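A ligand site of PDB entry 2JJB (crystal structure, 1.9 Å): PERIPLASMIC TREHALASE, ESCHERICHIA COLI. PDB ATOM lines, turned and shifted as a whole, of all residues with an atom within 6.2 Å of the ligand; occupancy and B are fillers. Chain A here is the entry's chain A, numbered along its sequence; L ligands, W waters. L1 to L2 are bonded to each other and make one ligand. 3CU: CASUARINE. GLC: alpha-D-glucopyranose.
OD2 of Asp 130 sits at hydrogen-bond distance from O2 of 3CU L1 (2.5 Å). The indole nitrogen of Trp 129 lies within hydrogen-bond range of an oxygen (O1) of 3CU L1, 3.0 Å away. NH1 of Arg 122 sits at hydrogen-bond distance from O6 of GLC L2 (2.7 Å). An oxygen (O3) of GLC L2 sits at hydrogen-bond distance from the side-chain amide oxygen (OD1) of Asn 166 (2.7 Å). The backbone carbonyl oxygen (O) of Gly 280 sits at hydrogen-bond distance from an oxygen (O1) of 3CU L1. An oxygen (O2) of 3CU L1 lies within hydrogen-bond range of the side-chain amide nitrogen of Gln 177. An oxygen (O3) of GLC L2 lies within hydrogen-bond range of the guanidinium group of Arg 175 (2.7 Å). NE1 of Trp 417 lies within hydrogen-bond range of O7 of 3CU L1. The guanidinium group (NH1) of Arg 247 is in hydrogen-bond range of an oxygen (O4) of GLC L2 (2.8 Å). An oxygen (O4) of GLC L2 is in hydrogen-bond range of the side-chain carboxylate (OE2) of Glu 249, 2.7 Å away.
N of Trp 129 lies within hydrogen-bond range of OE1 of Gln 177 (3.1 Å). The side-chain carboxylate (OE2) of Glu 249 is in salt-bridge range of the guanidinium group (NH2) of Arg 175, 2.9 Å away. O of Glu 249 sits at hydrogen-bond distance from N of Lys 31 (3.5 Å). The side-chain hydroxyl (OH) of Tyr 482 is in hydrogen-bond range of the side-chain amide nitrogen (NE2) of Gln 416 (3.0 Å). The indole nitrogen (NE1) of Trp 490 lies within hydrogen-bond range of the backbone carbonyl oxygen (O) of Glu 466, at 3.3 Å. The side-chain amino group (NZ) of Lys 31 is in hydrogen-bond range of the backbone carbonyl oxygen (O) of Arg 122, 3.0 Å away. OD1 of Asn 166 lies within hydrogen-bond range of NE of Arg 175 (2.9 Å). The side-chain amide nitrogen (NE2) of Gln 177 sits close to the side-chain amide nitrogen (ND2) of Asn 166 (3.2 Å).
Water W1 lies within hydrogen-bond range of the backbone carbonyl oxygen (O) of Ala 277 (2.7 Å), the side-chain carboxylate (OD1) of Asp 282 (2.7 Å), an oxygen (O2) of GLC L2 (2.8 Å) and the side-chain amide nitrogen (NE2) of Gln 177 (3.2 Å). Water W3 bridges the side-chain carboxylate of Glu 466 (2.7 Å) and an oxygen (O8) of 3CU L1 (2.8 Å). Water W2 lies within hydrogen-bond range of O of Asp 282, NE2 of Gln 416 and O7 of 3CU L1.
The side-chain carboxylate (OD2) of Asp 282 lies close to an oxygen (O1) of GLC L2, 3.3 Å away. Merely in contact with the ligand: Tyr 172 (3.3 Å), Phe 123 (3.3 Å), Tyr 482 (3.4 Å), Phe 488 (3.4 Å), Tyr 127 (3.4 Å), Trp 490 (3.5 Å), Gln 416 (3.5 Å), Ala 277 (3.5 Å) and Ser 250 (3.8 Å). 20 residues have an atom within 4 Å of the ligand: Arg 122, Phe 123, Tyr 127, Trp 129, Asp 130, Asn 166, Tyr 172, Arg 175, Gln 177, Arg 247, Glu 249, Ser 250, Ala 277, Gly 280, Asp 282, Gln 416, Trp 417, Tyr 482, Phe 488 and Trp 490.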
ATOM      1  N   LYS A  31     -22.120  20.248  16.099  1.00  0.00           N
ATOM      2  CA  LYS A  31     -21.312  19.434  17.041  1.00  0.00           C
ATOM      3  C   LYS A  31     -22.018  19.274  18.403  1.00  0.00           C
ATOM      4  O   LYS A  31     -21.789  18.299  19.105  1.00  0.00           O
ATOM      5  CB  LYS A  31     -19.921  20.056  17.256  1.00  0.00           C
ATOM      6  CG  LYS A  31     -18.915  19.132  17.996  1.00  0.00           C
ATOM      7  CD  LYS A  31     -17.486  19.655  17.847  1.00  0.00           C
ATOM      8  CE  LYS A  31     -16.479  18.740  18.543  1.00  0.00           C
ATOM      9  NZ  LYS A  31     -16.829  18.566  20.019  1.00  0.00           N
ATOM     10  N   PRO A 119      -7.935  21.567  22.558  1.00  0.00           N
ATOM     11  CA  PRO A 119      -7.575  22.806  21.867  1.00  0.00           C
ATOM     12  C   PRO A 119      -8.242  24.044  22.497  1.00  0.00           C
ATOM     13  O   PRO A 119      -7.605  25.085  22.627  1.00  0.00           O
ATOM     14  CB  PRO A 119      -8.129  22.575  20.452  1.00  0.00           C
ATOM     15  CG  PRO A 119      -8.119  21.089  20.249  1.00  0.00           C
ATOM     16  CD  PRO A 119      -8.466  20.547  21.636  1.00  0.00           C
ATOM     17  N   ARG A 122     -15.270  24.817  21.414  1.00  0.00           N
ATOM     18  CA  ARG A 122     -16.100  23.673  21.029  1.00  0.00           C
ATOM     19  C   ARG A 122     -15.279  22.389  20.929  1.00  0.00           C
ATOM     20  O   ARG A 122     -15.843  21.310  20.782  1.00  0.00           O
ATOM     21  CB  ARG A 122     -16.784  23.948  19.666  1.00  0.00           C
ATOM     22  CG  ARG A 122     -15.781  23.988  18.505  1.00  0.00           C
ATOM     23  CD  ARG A 122     -16.346  24.615  17.245  1.00  0.00           C
ATOM     24  NE  ARG A 122     -17.411  23.860  16.599  1.00  0.00           N
ATOM     25  CZ  ARG A 122     -17.264  23.012  15.581  1.00  0.00           C
ATOM     26  NH1 ARG A 122     -16.061  22.727  15.108  1.00  0.00           N
ATOM     27  NH2 ARG A 122     -18.327  22.436  15.031  1.00  0.00           N
ATOM     28  N   PHE A 123     -13.943  22.511  20.973  1.00  0.00           N
ATOM     29  CA  PHE A 123     -13.071  21.318  20.833  1.00  0.00           C
ATOM     30  C   PHE A 123     -12.788  20.769  22.209  1.00  0.00           C
ATOM     31  O   PHE A 123     -11.783  21.121  22.846  1.00  0.00           O
ATOM     32  CB  PHE A 123     -11.815  21.633  19.993  1.00  0.00           C
ATOM     33  CG  PHE A 123     -12.156  22.213  18.635  1.00  0.00           C
ATOM     34  CD1 PHE A 123     -12.796  21.429  17.679  1.00  0.00           C
ATOM     35  CD2 PHE A 123     -11.881  23.540  18.333  1.00  0.00           C
ATOM     36  CE1 PHE A 123     -13.156  21.966  16.452  1.00  0.00           C
ATOM     37  CE2 PHE A 123     -12.229  24.073  17.099  1.00  0.00           C
ATOM     38  CZ  PHE A 123     -12.860  23.297  16.156  1.00  0.00           C
ATOM     39  N   TYR A 127      -7.189  16.154  20.286  1.00  0.00           N
ATOM     40  CA  TYR A 127      -7.057  16.091  18.833  1.00  0.00           C
ATOM     41  C   TYR A 127      -5.679  15.540  18.535  1.00  0.00           C
ATOM     42  O   TYR A 127      -4.746  15.832  19.265  1.00  0.00           O
ATOM     43  CB  TYR A 127      -7.288  17.465  18.164  1.00  0.00           C
ATOM     44  CG  TYR A 127      -8.759  17.708  18.026  1.00  0.00           C
ATOM     45  CD1 TYR A 127      -9.515  18.042  19.138  1.00  0.00           C
ATOM     46  CD2 TYR A 127      -9.413  17.523  16.807  1.00  0.00           C
ATOM     47  CE1 TYR A 127     -10.894  18.206  19.063  1.00  0.00           C
ATOM     48  CE2 TYR A 127     -10.832  17.696  16.717  1.00  0.00           C
ATOM     49  CZ  TYR A 127     -11.542  18.036  17.862  1.00  0.00           C
ATOM     50  OH  TYR A 127     -12.904  18.151  17.825  1.00  0.00           O
ATOM     51  N   TYR A 128      -5.568  14.732  17.481  1.00  0.00           N
ATOM     52  CA  TYR A 128      -4.304  14.054  17.203  1.00  0.00           C
ATOM     53  C   TYR A 128      -3.208  15.032  16.813  1.00  0.00           C
ATOM     54  O   TYR A 128      -2.286  15.220  17.584  1.00  0.00           O
ATOM     55  CB  TYR A 128      -4.483  12.966  16.139  1.00  0.00           C
ATOM     56  CG  TYR A 128      -3.272  12.111  15.824  1.00  0.00           C
ATOM     57  CD1 TYR A 128      -2.084  12.147  16.602  1.00  0.00           C
ATOM     58  CD2 TYR A 128      -3.327  11.184  14.769  1.00  0.00           C
ATOM     59  CE1 TYR A 128      -0.990  11.329  16.298  1.00  0.00           C
ATOM     60  CE2 TYR A 128      -2.254  10.365  14.473  1.00  0.00           C
ATOM     61  CZ  TYR A 128      -1.101  10.444  15.230  1.00  0.00           C
ATOM     62  OH  TYR A 128      -0.077   9.600  14.889  1.00  0.00           O
ATOM     63  N   TRP A 129      -3.266  15.675  15.635  1.00  0.00           N
ATOM     64  CA  TRP A 129      -2.085  16.472  15.298  1.00  0.00           C
ATOM     65  C   TRP A 129      -1.912  17.741  16.126  1.00  0.00           C
ATOM     66  O   TRP A 129      -0.764  18.122  16.408  1.00  0.00           O
ATOM     67  CB  TRP A 129      -1.913  16.701  13.781  1.00  0.00           C
ATOM     68  CG  TRP A 129      -2.835  17.716  13.085  1.00  0.00           C
ATOM     69  CD1 TRP A 129      -4.185  17.906  13.263  1.00  0.00           C
ATOM     70  CD2 TRP A 129      -2.447  18.601  12.028  1.00  0.00           C
ATOM     71  NE1 TRP A 129      -4.650  18.883  12.388  1.00  0.00           N
ATOM     72  CE2 TRP A 129      -3.603  19.321  11.626  1.00  0.00           C
ATOM     73  CE3 TRP A 129      -1.213  18.852  11.396  1.00  0.00           C
ATOM     74  CZ2 TRP A 129      -3.563  20.307  10.604  1.00  0.00           C
ATOM     75  CZ3 TRP A 129      -1.164  19.844  10.387  1.00  0.00           C
ATOM     76  CH2 TRP A 129      -2.343  20.547   9.996  1.00  0.00           C
ATOM     77  N   ASP A 130      -3.026  18.342  16.580  1.00  0.00           N
ATOM     78  CA  ASP A 130      -2.954  19.512  17.466  1.00  0.00           C
ATOM     79  C   ASP A 130      -2.093  19.156  18.665  1.00  0.00           C
ATOM     80  O   ASP A 130      -1.340  19.983  19.163  1.00  0.00           O
ATOM     81  CB  ASP A 130      -4.309  19.887  18.070  1.00  0.00           C
ATOM     82  CG  ASP A 130      -5.334  20.273  17.021  1.00  0.00           C
ATOM     83  OD1 ASP A 130      -5.889  21.381  17.124  1.00  0.00           O
ATOM     84  OD2 ASP A 130      -5.591  19.432  16.129  1.00  0.00           O
ATOM     85  N   ASN A 166      -9.030  10.735  15.007  1.00  0.00           N
ATOM     86  CA  ASN A 166      -8.996  12.195  14.839  1.00  0.00           C
ATOM     87  C   ASN A 166      -9.059  12.877  16.231  1.00  0.00           C
ATOM     88  O   ASN A 166      -8.344  13.836  16.490  1.00  0.00           O
ATOM     89  CB  ASN A 166     -10.174  12.584  13.931  1.00  0.00           C
ATOM     90  CG  ASN A 166     -10.239  14.067  13.495  1.00  0.00           C
ATOM     91  OD1 ASN A 166     -10.839  14.322  12.472  1.00  0.00           O
ATOM     92  ND2 ASN A 166      -9.771  15.024  14.294  1.00  0.00           N
ATOM     93  N   TYR A 172     -15.255  10.195  15.572  1.00  0.00           N
ATOM     94  CA  TYR A 172     -13.929  10.313  14.970  1.00  0.00           C
ATOM     95  C   TYR A 172     -13.188   8.993  14.807  1.00  0.00           C
ATOM     96  O   TYR A 172     -12.061   8.996  14.318  1.00  0.00           O
ATOM     97  CB  TYR A 172     -13.034  11.196  15.841  1.00  0.00           C
ATOM     98  CG  TYR A 172     -13.376  12.674  15.869  1.00  0.00           C
ATOM     99  CD1 TYR A 172     -13.897  13.315  14.749  1.00  0.00           C
ATOM    100  CD2 TYR A 172     -13.068  13.445  16.996  1.00  0.00           C
ATOM    101  CE1 TYR A 172     -14.171  14.672  14.761  1.00  0.00           C
ATOM    102  CE2 TYR A 172     -13.338  14.821  17.018  1.00  0.00           C
ATOM    103  CZ  TYR A 172     -13.883  15.415  15.879  1.00  0.00           C
ATOM    104  OH  TYR A 172     -14.197  16.749  15.832  1.00  0.00           O
ATOM    105  N   ARG A 175     -11.506   7.435  11.406  1.00  0.00           N
ATOM    106  CA  ARG A 175     -10.376   8.064  10.713  1.00  0.00           C
ATOM    107  C   ARG A 175      -9.278   8.380  11.700  1.00  0.00           C
ATOM    108  O   ARG A 175      -9.500   8.288  12.898  1.00  0.00           O
ATOM    109  CB  ARG A 175     -10.820   9.321   9.950  1.00  0.00           C
ATOM    110  CG  ARG A 175     -11.498  10.418  10.823  1.00  0.00           C
ATOM    111  CD  ARG A 175     -11.687  11.666   9.996  1.00  0.00           C
ATOM    112  NE  ARG A 175     -12.470  12.736  10.646  1.00  0.00           N
ATOM    113  CZ  ARG A 175     -13.800  12.809  10.695  1.00  0.00           C
ATOM    114  NH1 ARG A 175     -14.584  11.836  10.182  1.00  0.00           N
ATOM    115  NH2 ARG A 175     -14.349  13.869  11.290  1.00  0.00           N
ATOM    116  N   GLN A 177      -5.544  11.151  11.662  1.00  0.00           N
ATOM    117  CA  GLN A 177      -5.216  12.531  11.370  1.00  0.00           C
ATOM    118  C   GLN A 177      -3.739  12.528  10.966  1.00  0.00           C
ATOM    119  O   GLN A 177      -3.146  11.453  10.941  1.00  0.00           O
ATOM    120  CB  GLN A 177      -5.478  13.459  12.586  1.00  0.00           C
ATOM    121  CG  GLN A 177      -6.591  14.482  12.276  1.00  0.00           C
ATOM    122  CD  GLN A 177      -6.640  15.646  13.246  1.00  0.00           C
ATOM    123  OE1 GLN A 177      -6.067  15.599  14.346  1.00  0.00           O
ATOM    124  NE2 GLN A 177      -7.392  16.688  12.857  1.00  0.00           N
ATOM    125  N   ARG A 247     -20.773  13.558   8.327  1.00  0.00           N
ATOM    126  CA  ARG A 247     -20.119  13.578   9.620  1.00  0.00           C
ATOM    127  C   ARG A 247     -21.160  13.997  10.667  1.00  0.00           C
ATOM    128  O   ARG A 247     -21.783  15.065  10.514  1.00  0.00           O
ATOM    129  CB  ARG A 247     -18.954  14.563   9.629  1.00  0.00           C
ATOM    130  CG  ARG A 247     -17.769  14.167   8.746  1.00  0.00           C
ATOM    131  CD  ARG A 247     -16.810  15.379   8.633  1.00  0.00           C
ATOM    132  NE  ARG A 247     -17.466  16.485   7.905  1.00  0.00           N
ATOM    133  CZ  ARG A 247     -17.060  17.754   7.898  1.00  0.00           C
ATOM    134  NH1 ARG A 247     -16.005  18.163   8.624  1.00  0.00           N
ATOM    135  NH2 ARG A 247     -17.756  18.648   7.182  1.00  0.00           N
ATOM    136  N   GLU A 249     -20.848  15.476  13.374  1.00  0.00           N
ATOM    137  CA  GLU A 249     -20.547  16.778  13.919  1.00  0.00           C
ATOM    138  C   GLU A 249     -20.740  17.892  12.887  1.00  0.00           C
ATOM    139  O   GLU A 249     -20.604  19.063  13.209  1.00  0.00           O
ATOM    140  CB  GLU A 249     -19.124  16.814  14.509  1.00  0.00           C
ATOM    141  CG  GLU A 249     -17.963  16.837  13.469  1.00  0.00           C
ATOM    142  CD  GLU A 249     -17.620  15.481  12.842  1.00  0.00           C
ATOM    143  OE1 GLU A 249     -18.386  14.478  12.990  1.00  0.00           O
ATOM    144  OE2 GLU A 249     -16.562  15.442  12.170  1.00  0.00           O
ATOM    145  N   SER A 250     -21.017  17.526  11.633  1.00  0.00           N
ATOM    146  CA  SER A 250     -21.236  18.521  10.552  1.00  0.00           C
ATOM    147  C   SER A 250     -22.371  18.048   9.646  1.00  0.00           C
ATOM    148  O   SER A 250     -22.337  18.261   8.403  1.00  0.00           O
ATOM    149  CB  SER A 250     -19.956  18.699   9.731  1.00  0.00           C
ATOM    150  OG  SER A 250     -18.867  19.037  10.548  1.00  0.00           O
ATOM    151  N   ALA A 277     -11.242  15.808   6.395  1.00  0.00           N
ATOM    152  CA  ALA A 277     -11.106  16.032   7.846  1.00  0.00           C
ATOM    153  C   ALA A 277      -9.957  15.161   8.421  1.00  0.00           C
ATOM    154  O   ALA A 277      -9.264  15.577   9.329  1.00  0.00           O
ATOM    155  CB  ALA A 277     -12.464  15.782   8.568  1.00  0.00           C
ATOM    156  N   ALA A 278      -9.730  13.966   7.855  1.00  0.00           N
ATOM    157  CA  ALA A 278      -8.592  13.127   8.280  1.00  0.00           C
ATOM    158  C   ALA A 278      -7.263  13.840   7.990  1.00  0.00           C
ATOM    159  O   ALA A 278      -6.277  13.714   8.754  1.00  0.00           O
ATOM    160  CB  ALA A 278      -8.649  11.750   7.598  1.00  0.00           C
ATOM    161  N   SER A 279      -7.227  14.638   6.917  1.00  0.00           N
ATOM    162  CA  SER A 279      -5.977  15.346   6.508  1.00  0.00           C
ATOM    163  C   SER A 279      -5.680  16.536   7.398  1.00  0.00           C
ATOM    164  O   SER A 279      -4.581  17.089   7.332  1.00  0.00           O
ATOM    165  CB  SER A 279      -6.105  15.884   5.072  1.00  0.00           C
ATOM    166  OG  SER A 279      -6.904  17.049   5.064  1.00  0.00           O
ATOM    167  N   GLY A 280      -6.666  16.941   8.201  1.00  0.00           N
ATOM    168  CA  GLY A 280      -6.567  18.153   9.014  1.00  0.00           C
ATOM    169  C   GLY A 280      -7.007  19.408   8.273  1.00  0.00           C
ATOM    170  O   GLY A 280      -7.430  20.400   8.898  1.00  0.00           O
ATOM    171  N   TRP A 281      -6.919  19.352   6.942  1.00  0.00           N
ATOM    172  CA  TRP A 281      -7.227  20.520   6.105  1.00  0.00           C
ATOM    173  C   TRP A 281      -8.666  20.464   5.583  1.00  0.00           C
ATOM    174  O   TRP A 281      -8.894  20.419   4.368  1.00  0.00           O
ATOM    175  CB  TRP A 281      -6.258  20.582   4.933  1.00  0.00           C
ATOM    176  CG  TRP A 281      -4.802  20.843   5.235  1.00  0.00           C
ATOM    177  CD1 TRP A 281      -4.013  20.259   6.214  1.00  0.00           C
ATOM    178  CD2 TRP A 281      -3.939  21.704   4.485  1.00  0.00           C
ATOM    179  NE1 TRP A 281      -2.714  20.740   6.120  1.00  0.00           N
ATOM    180  CE2 TRP A 281      -2.640  21.627   5.072  1.00  0.00           C
ATOM    181  CE3 TRP A 281      -4.138  22.559   3.373  1.00  0.00           C
ATOM    182  CZ2 TRP A 281      -1.542  22.370   4.575  1.00  0.00           C
ATOM    183  CZ3 TRP A 281      -3.049  23.298   2.877  1.00  0.00           C
ATOM    184  CH2 TRP A 281      -1.773  23.179   3.472  1.00  0.00           C
ATOM    185  N   ASP A 282      -9.644  20.426   6.499  1.00  0.00           N
ATOM    186  CA  ASP A 282     -11.051  20.518   6.092  1.00  0.00           C
ATOM    187  C   ASP A 282     -11.470  22.008   6.185  1.00  0.00           C
ATOM    188  O   ASP A 282     -11.629  22.496   7.300  1.00  0.00           O
ATOM    189  CB  ASP A 282     -11.970  19.645   6.983  1.00  0.00           C
ATOM    190  CG  ASP A 282     -11.700  19.795   8.494  1.00  0.00           C
ATOM    191  OD1 ASP A 282     -10.586  19.485   8.929  1.00  0.00           O
ATOM    192  OD2 ASP A 282     -12.613  20.222   9.255  1.00  0.00           O
ATOM    193  N   PHE A 283     -11.645  22.724   5.076  1.00  0.00           N
ATOM    194  CA  PHE A 283     -11.414  22.273   3.693  1.00  0.00           C
ATOM    195  C   PHE A 283     -10.415  23.156   2.949  1.00  0.00           C
ATOM    196  O   PHE A 283      -9.982  24.184   3.469  1.00  0.00           O
ATOM    197  CB  PHE A 283     -12.762  22.134   2.932  1.00  0.00           C
ATOM    198  CG  PHE A 283     -13.662  21.116   3.576  1.00  0.00           C
ATOM    199  CD1 PHE A 283     -13.389  19.757   3.464  1.00  0.00           C
ATOM    200  CD2 PHE A 283     -14.738  21.525   4.396  1.00  0.00           C
ATOM    201  CE1 PHE A 283     -14.163  18.805   4.120  1.00  0.00           C
ATOM    202  CE2 PHE A 283     -15.546  20.570   5.039  1.00  0.00           C
ATOM    203  CZ  PHE A 283     -15.240  19.210   4.912  1.00  0.00           C
ATOM    204  N   GLN A 416     -11.315  27.254   5.091  1.00  0.00           N
ATOM    205  CA  GLN A 416     -10.441  27.499   6.242  1.00  0.00           C
ATOM    206  C   GLN A 416      -8.972  27.201   5.972  1.00  0.00           C
ATOM    207  O   GLN A 416      -8.084  27.931   6.441  1.00  0.00           O
ATOM    208  CB  GLN A 416     -10.919  26.698   7.451  1.00  0.00           C
ATOM    209  CG  GLN A 416     -12.065  27.360   8.168  1.00  0.00           C
ATOM    210  CD  GLN A 416     -11.924  27.227   9.686  1.00  0.00           C
ATOM    211  OE1 GLN A 416     -11.508  28.169  10.360  1.00  0.00           O
ATOM    212  NE2 GLN A 416     -12.243  26.044  10.206  1.00  0.00           N
ATOM    213  N   TRP A 417      -8.685  26.133   5.222  1.00  0.00           N
ATOM    214  CA  TRP A 417      -7.283  25.769   4.952  1.00  0.00           C
ATOM    215  C   TRP A 417      -6.814  26.322   3.596  1.00  0.00           C
ATOM    216  O   TRP A 417      -6.486  25.582   2.667  1.00  0.00           O
ATOM    217  CB  TRP A 417      -7.091  24.249   5.175  1.00  0.00           C
ATOM    218  CG  TRP A 417      -7.236  23.978   6.642  1.00  0.00           C
ATOM    219  CD1 TRP A 417      -8.404  23.863   7.354  1.00  0.00           C
ATOM    220  CD2 TRP A 417      -6.181  23.870   7.587  1.00  0.00           C
ATOM    221  NE1 TRP A 417      -8.142  23.666   8.693  1.00  0.00           N
ATOM    222  CE2 TRP A 417      -6.781  23.680   8.872  1.00  0.00           C
ATOM    223  CE3 TRP A 417      -4.776  23.882   7.484  1.00  0.00           C
ATOM    224  CZ2 TRP A 417      -6.028  23.508  10.019  1.00  0.00           C
ATOM    225  CZ3 TRP A 417      -4.019  23.708   8.653  1.00  0.00           C
ATOM    226  CH2 TRP A 417      -4.651  23.529   9.908  1.00  0.00           C
ATOM    227  N   TRP A 423      -2.178  29.151  10.019  1.00  0.00           N
ATOM    228  CA  TRP A 423      -2.392  28.160  11.062  1.00  0.00           C
ATOM    229  C   TRP A 423      -1.064  27.865  11.739  1.00  0.00           C
ATOM    230  O   TRP A 423      -0.105  27.500  11.058  1.00  0.00           O
ATOM    231  CB  TRP A 423      -2.953  26.884  10.419  1.00  0.00           C
ATOM    232  CG  TRP A 423      -4.394  27.028   9.947  1.00  0.00           C
ATOM    233  CD1 TRP A 423      -4.832  27.401   8.702  1.00  0.00           C
ATOM    234  CD2 TRP A 423      -5.575  26.823  10.734  1.00  0.00           C
ATOM    235  NE1 TRP A 423      -6.221  27.413   8.663  1.00  0.00           N
ATOM    236  CE2 TRP A 423      -6.696  27.069   9.901  1.00  0.00           C
ATOM    237  CE3 TRP A 423      -5.795  26.444  12.079  1.00  0.00           C
ATOM    238  CZ2 TRP A 423      -8.017  26.930  10.364  1.00  0.00           C
ATOM    239  CZ3 TRP A 423      -7.077  26.290  12.529  1.00  0.00           C
ATOM    240  CH2 TRP A 423      -8.201  26.539  11.674  1.00  0.00           C
ATOM    241  N   GLU A 466      -7.597  29.992  17.074  1.00  0.00           N
ATOM    242  CA  GLU A 466      -7.253  28.813  16.256  1.00  0.00           C
ATOM    243  C   GLU A 466      -6.401  29.167  15.026  1.00  0.00           C
ATOM    244  O   GLU A 466      -5.514  28.377  14.615  1.00  0.00           O
ATOM    245  CB  GLU A 466      -8.497  27.961  15.950  1.00  0.00           C
ATOM    246  CG  GLU A 466      -9.504  28.553  15.056  1.00  0.00           C
ATOM    247  CD  GLU A 466     -10.808  27.763  14.964  1.00  0.00           C
ATOM    248  OE1 GLU A 466     -10.795  26.515  14.731  1.00  0.00           O
ATOM    249  OE2 GLU A 466     -11.862  28.439  15.027  1.00  0.00           O
ATOM    250  N   TYR A 482     -18.439  27.452  11.765  1.00  0.00           N
ATOM    251  CA  TYR A 482     -18.576  27.614  13.207  1.00  0.00           C
ATOM    252  C   TYR A 482     -17.762  28.870  13.543  1.00  0.00           C
ATOM    253  O   TYR A 482     -16.866  29.211  12.811  1.00  0.00           O
ATOM    254  CB  TYR A 482     -18.070  26.363  13.960  1.00  0.00           C
ATOM    255  CG  TYR A 482     -16.602  26.057  13.735  1.00  0.00           C
ATOM    256  CD1 TYR A 482     -15.621  26.691  14.493  1.00  0.00           C
ATOM    257  CD2 TYR A 482     -16.192  25.145  12.778  1.00  0.00           C
ATOM    258  CE1 TYR A 482     -14.279  26.445  14.296  1.00  0.00           C
ATOM    259  CE2 TYR A 482     -14.838  24.874  12.586  1.00  0.00           C
ATOM    260  CZ  TYR A 482     -13.897  25.544  13.346  1.00  0.00           C
ATOM    261  OH  TYR A 482     -12.553  25.339  13.149  1.00  0.00           O
ATOM    262  N   PHE A 488      -5.388  28.825  22.517  1.00  0.00           N
ATOM    263  CA  PHE A 488      -5.872  27.743  21.648  1.00  0.00           C
ATOM    264  C   PHE A 488      -4.680  26.806  21.479  1.00  0.00           C
ATOM    265  O   PHE A 488      -3.614  27.253  21.089  1.00  0.00           O
ATOM    266  CB  PHE A 488      -6.359  28.228  20.269  1.00  0.00           C
ATOM    267  CG  PHE A 488      -7.121  27.153  19.523  1.00  0.00           C
ATOM    268  CD1 PHE A 488      -8.485  26.954  19.768  1.00  0.00           C
ATOM    269  CD2 PHE A 488      -6.467  26.305  18.626  1.00  0.00           C
ATOM    270  CE1 PHE A 488      -9.185  25.936  19.117  1.00  0.00           C
ATOM    271  CE2 PHE A 488      -7.152  25.278  17.977  1.00  0.00           C
ATOM    272  CZ  PHE A 488      -8.514  25.118  18.207  1.00  0.00           C
ATOM    273  N   TRP A 490      -2.722  24.483  19.812  1.00  0.00           N
ATOM    274  CA  TRP A 490      -1.506  24.540  18.994  1.00  0.00           C
ATOM    275  C   TRP A 490      -0.933  25.929  18.816  1.00  0.00           C
ATOM    276  O   TRP A 490       0.259  26.061  18.553  1.00  0.00           O
ATOM    277  CB  TRP A 490      -1.638  23.851  17.630  1.00  0.00           C
ATOM    278  CG  TRP A 490      -2.748  24.277  16.692  1.00  0.00           C
ATOM    279  CD1 TRP A 490      -3.428  25.484  16.622  1.00  0.00           C
ATOM    280  CD2 TRP A 490      -3.249  23.461  15.644  1.00  0.00           C
ATOM    281  NE1 TRP A 490      -4.378  25.419  15.576  1.00  0.00           N
ATOM    282  CE2 TRP A 490      -4.263  24.190  14.962  1.00  0.00           C
ATOM    283  CE3 TRP A 490      -2.919  22.155  15.203  1.00  0.00           C
ATOM    284  CZ2 TRP A 490      -4.950  23.650  13.875  1.00  0.00           C
ATOM    285  CZ3 TRP A 490      -3.656  21.608  14.134  1.00  0.00           C
ATOM    286  CH2 TRP A 490      -4.642  22.358  13.490  1.00  0.00           C
HETATM  287  O7  3CU L   1     -10.391  23.097  10.733  1.00  0.00           O
HETATM  288  C7  3CU L   1     -10.205  21.835  11.390  1.00  0.00           C
HETATM  289  C7A 3CU L   1      -8.972  21.946  12.282  1.00  0.00           C
HETATM  290  C1  3CU L   1      -8.152  20.653  12.414  1.00  0.00           C
HETATM  291  O1  3CU L   1      -7.007  20.621  11.572  1.00  0.00           O
HETATM  292  C2  3CU L   1      -7.767  20.585  13.905  1.00  0.00           C
HETATM  293  O2  3CU L   1      -7.391  19.268  14.336  1.00  0.00           O
HETATM  294  C3  3CU L   1      -9.090  20.942  14.598  1.00  0.00           C
HETATM  295  C8  3CU L   1      -8.983  21.389  16.073  1.00  0.00           C
HETATM  296  O8  3CU L   1      -8.075  22.450  16.212  1.00  0.00           O
HETATM  297  N4  3CU L   1      -9.629  21.875  13.589  1.00  0.00           N
HETATM  298  C5  3CU L   1     -10.977  22.405  13.588  1.00  0.00           C
HETATM  299  C6  3CU L   1     -11.417  21.616  12.332  1.00  0.00           C
HETATM  300  C1  GLC L   2     -12.160  19.497  13.395  1.00  0.00           C
HETATM  301  C2  GLC L   2     -12.058  17.965  13.299  1.00  0.00           C
HETATM  302  C3  GLC L   2     -12.863  17.431  12.092  1.00  0.00           C
HETATM  303  C4  GLC L   2     -14.326  17.914  12.248  1.00  0.00           C
HETATM  304  C5  GLC L   2     -14.381  19.436  12.330  1.00  0.00           C
HETATM  305  C6  GLC L   2     -15.802  19.973  12.589  1.00  0.00           C
HETATM  306  O1  GLC L   2     -11.435  20.158  12.370  1.00  0.00           O
HETATM  307  O2  GLC L   2     -10.692  17.601  13.282  1.00  0.00           O
HETATM  308  O3  GLC L   2     -12.836  16.026  12.068  1.00  0.00           O
HETATM  309  O4  GLC L   2     -15.122  17.440  11.173  1.00  0.00           O
HETATM  310  O5  GLC L   2     -13.519  19.903  13.360  1.00  0.00           O
HETATM  311  O6  GLC L   2     -15.801  21.399  12.738  1.00  0.00           O
HETATM  312  O   HOH W   1      -9.571  17.815  10.767  1.00  0.00           O
HETATM  313  O   HOH W   2     -12.838  23.563   9.389  1.00  0.00           O
HETATM  314  O   HOH W   3      -8.855  24.601  14.643  1.00  0.00           O
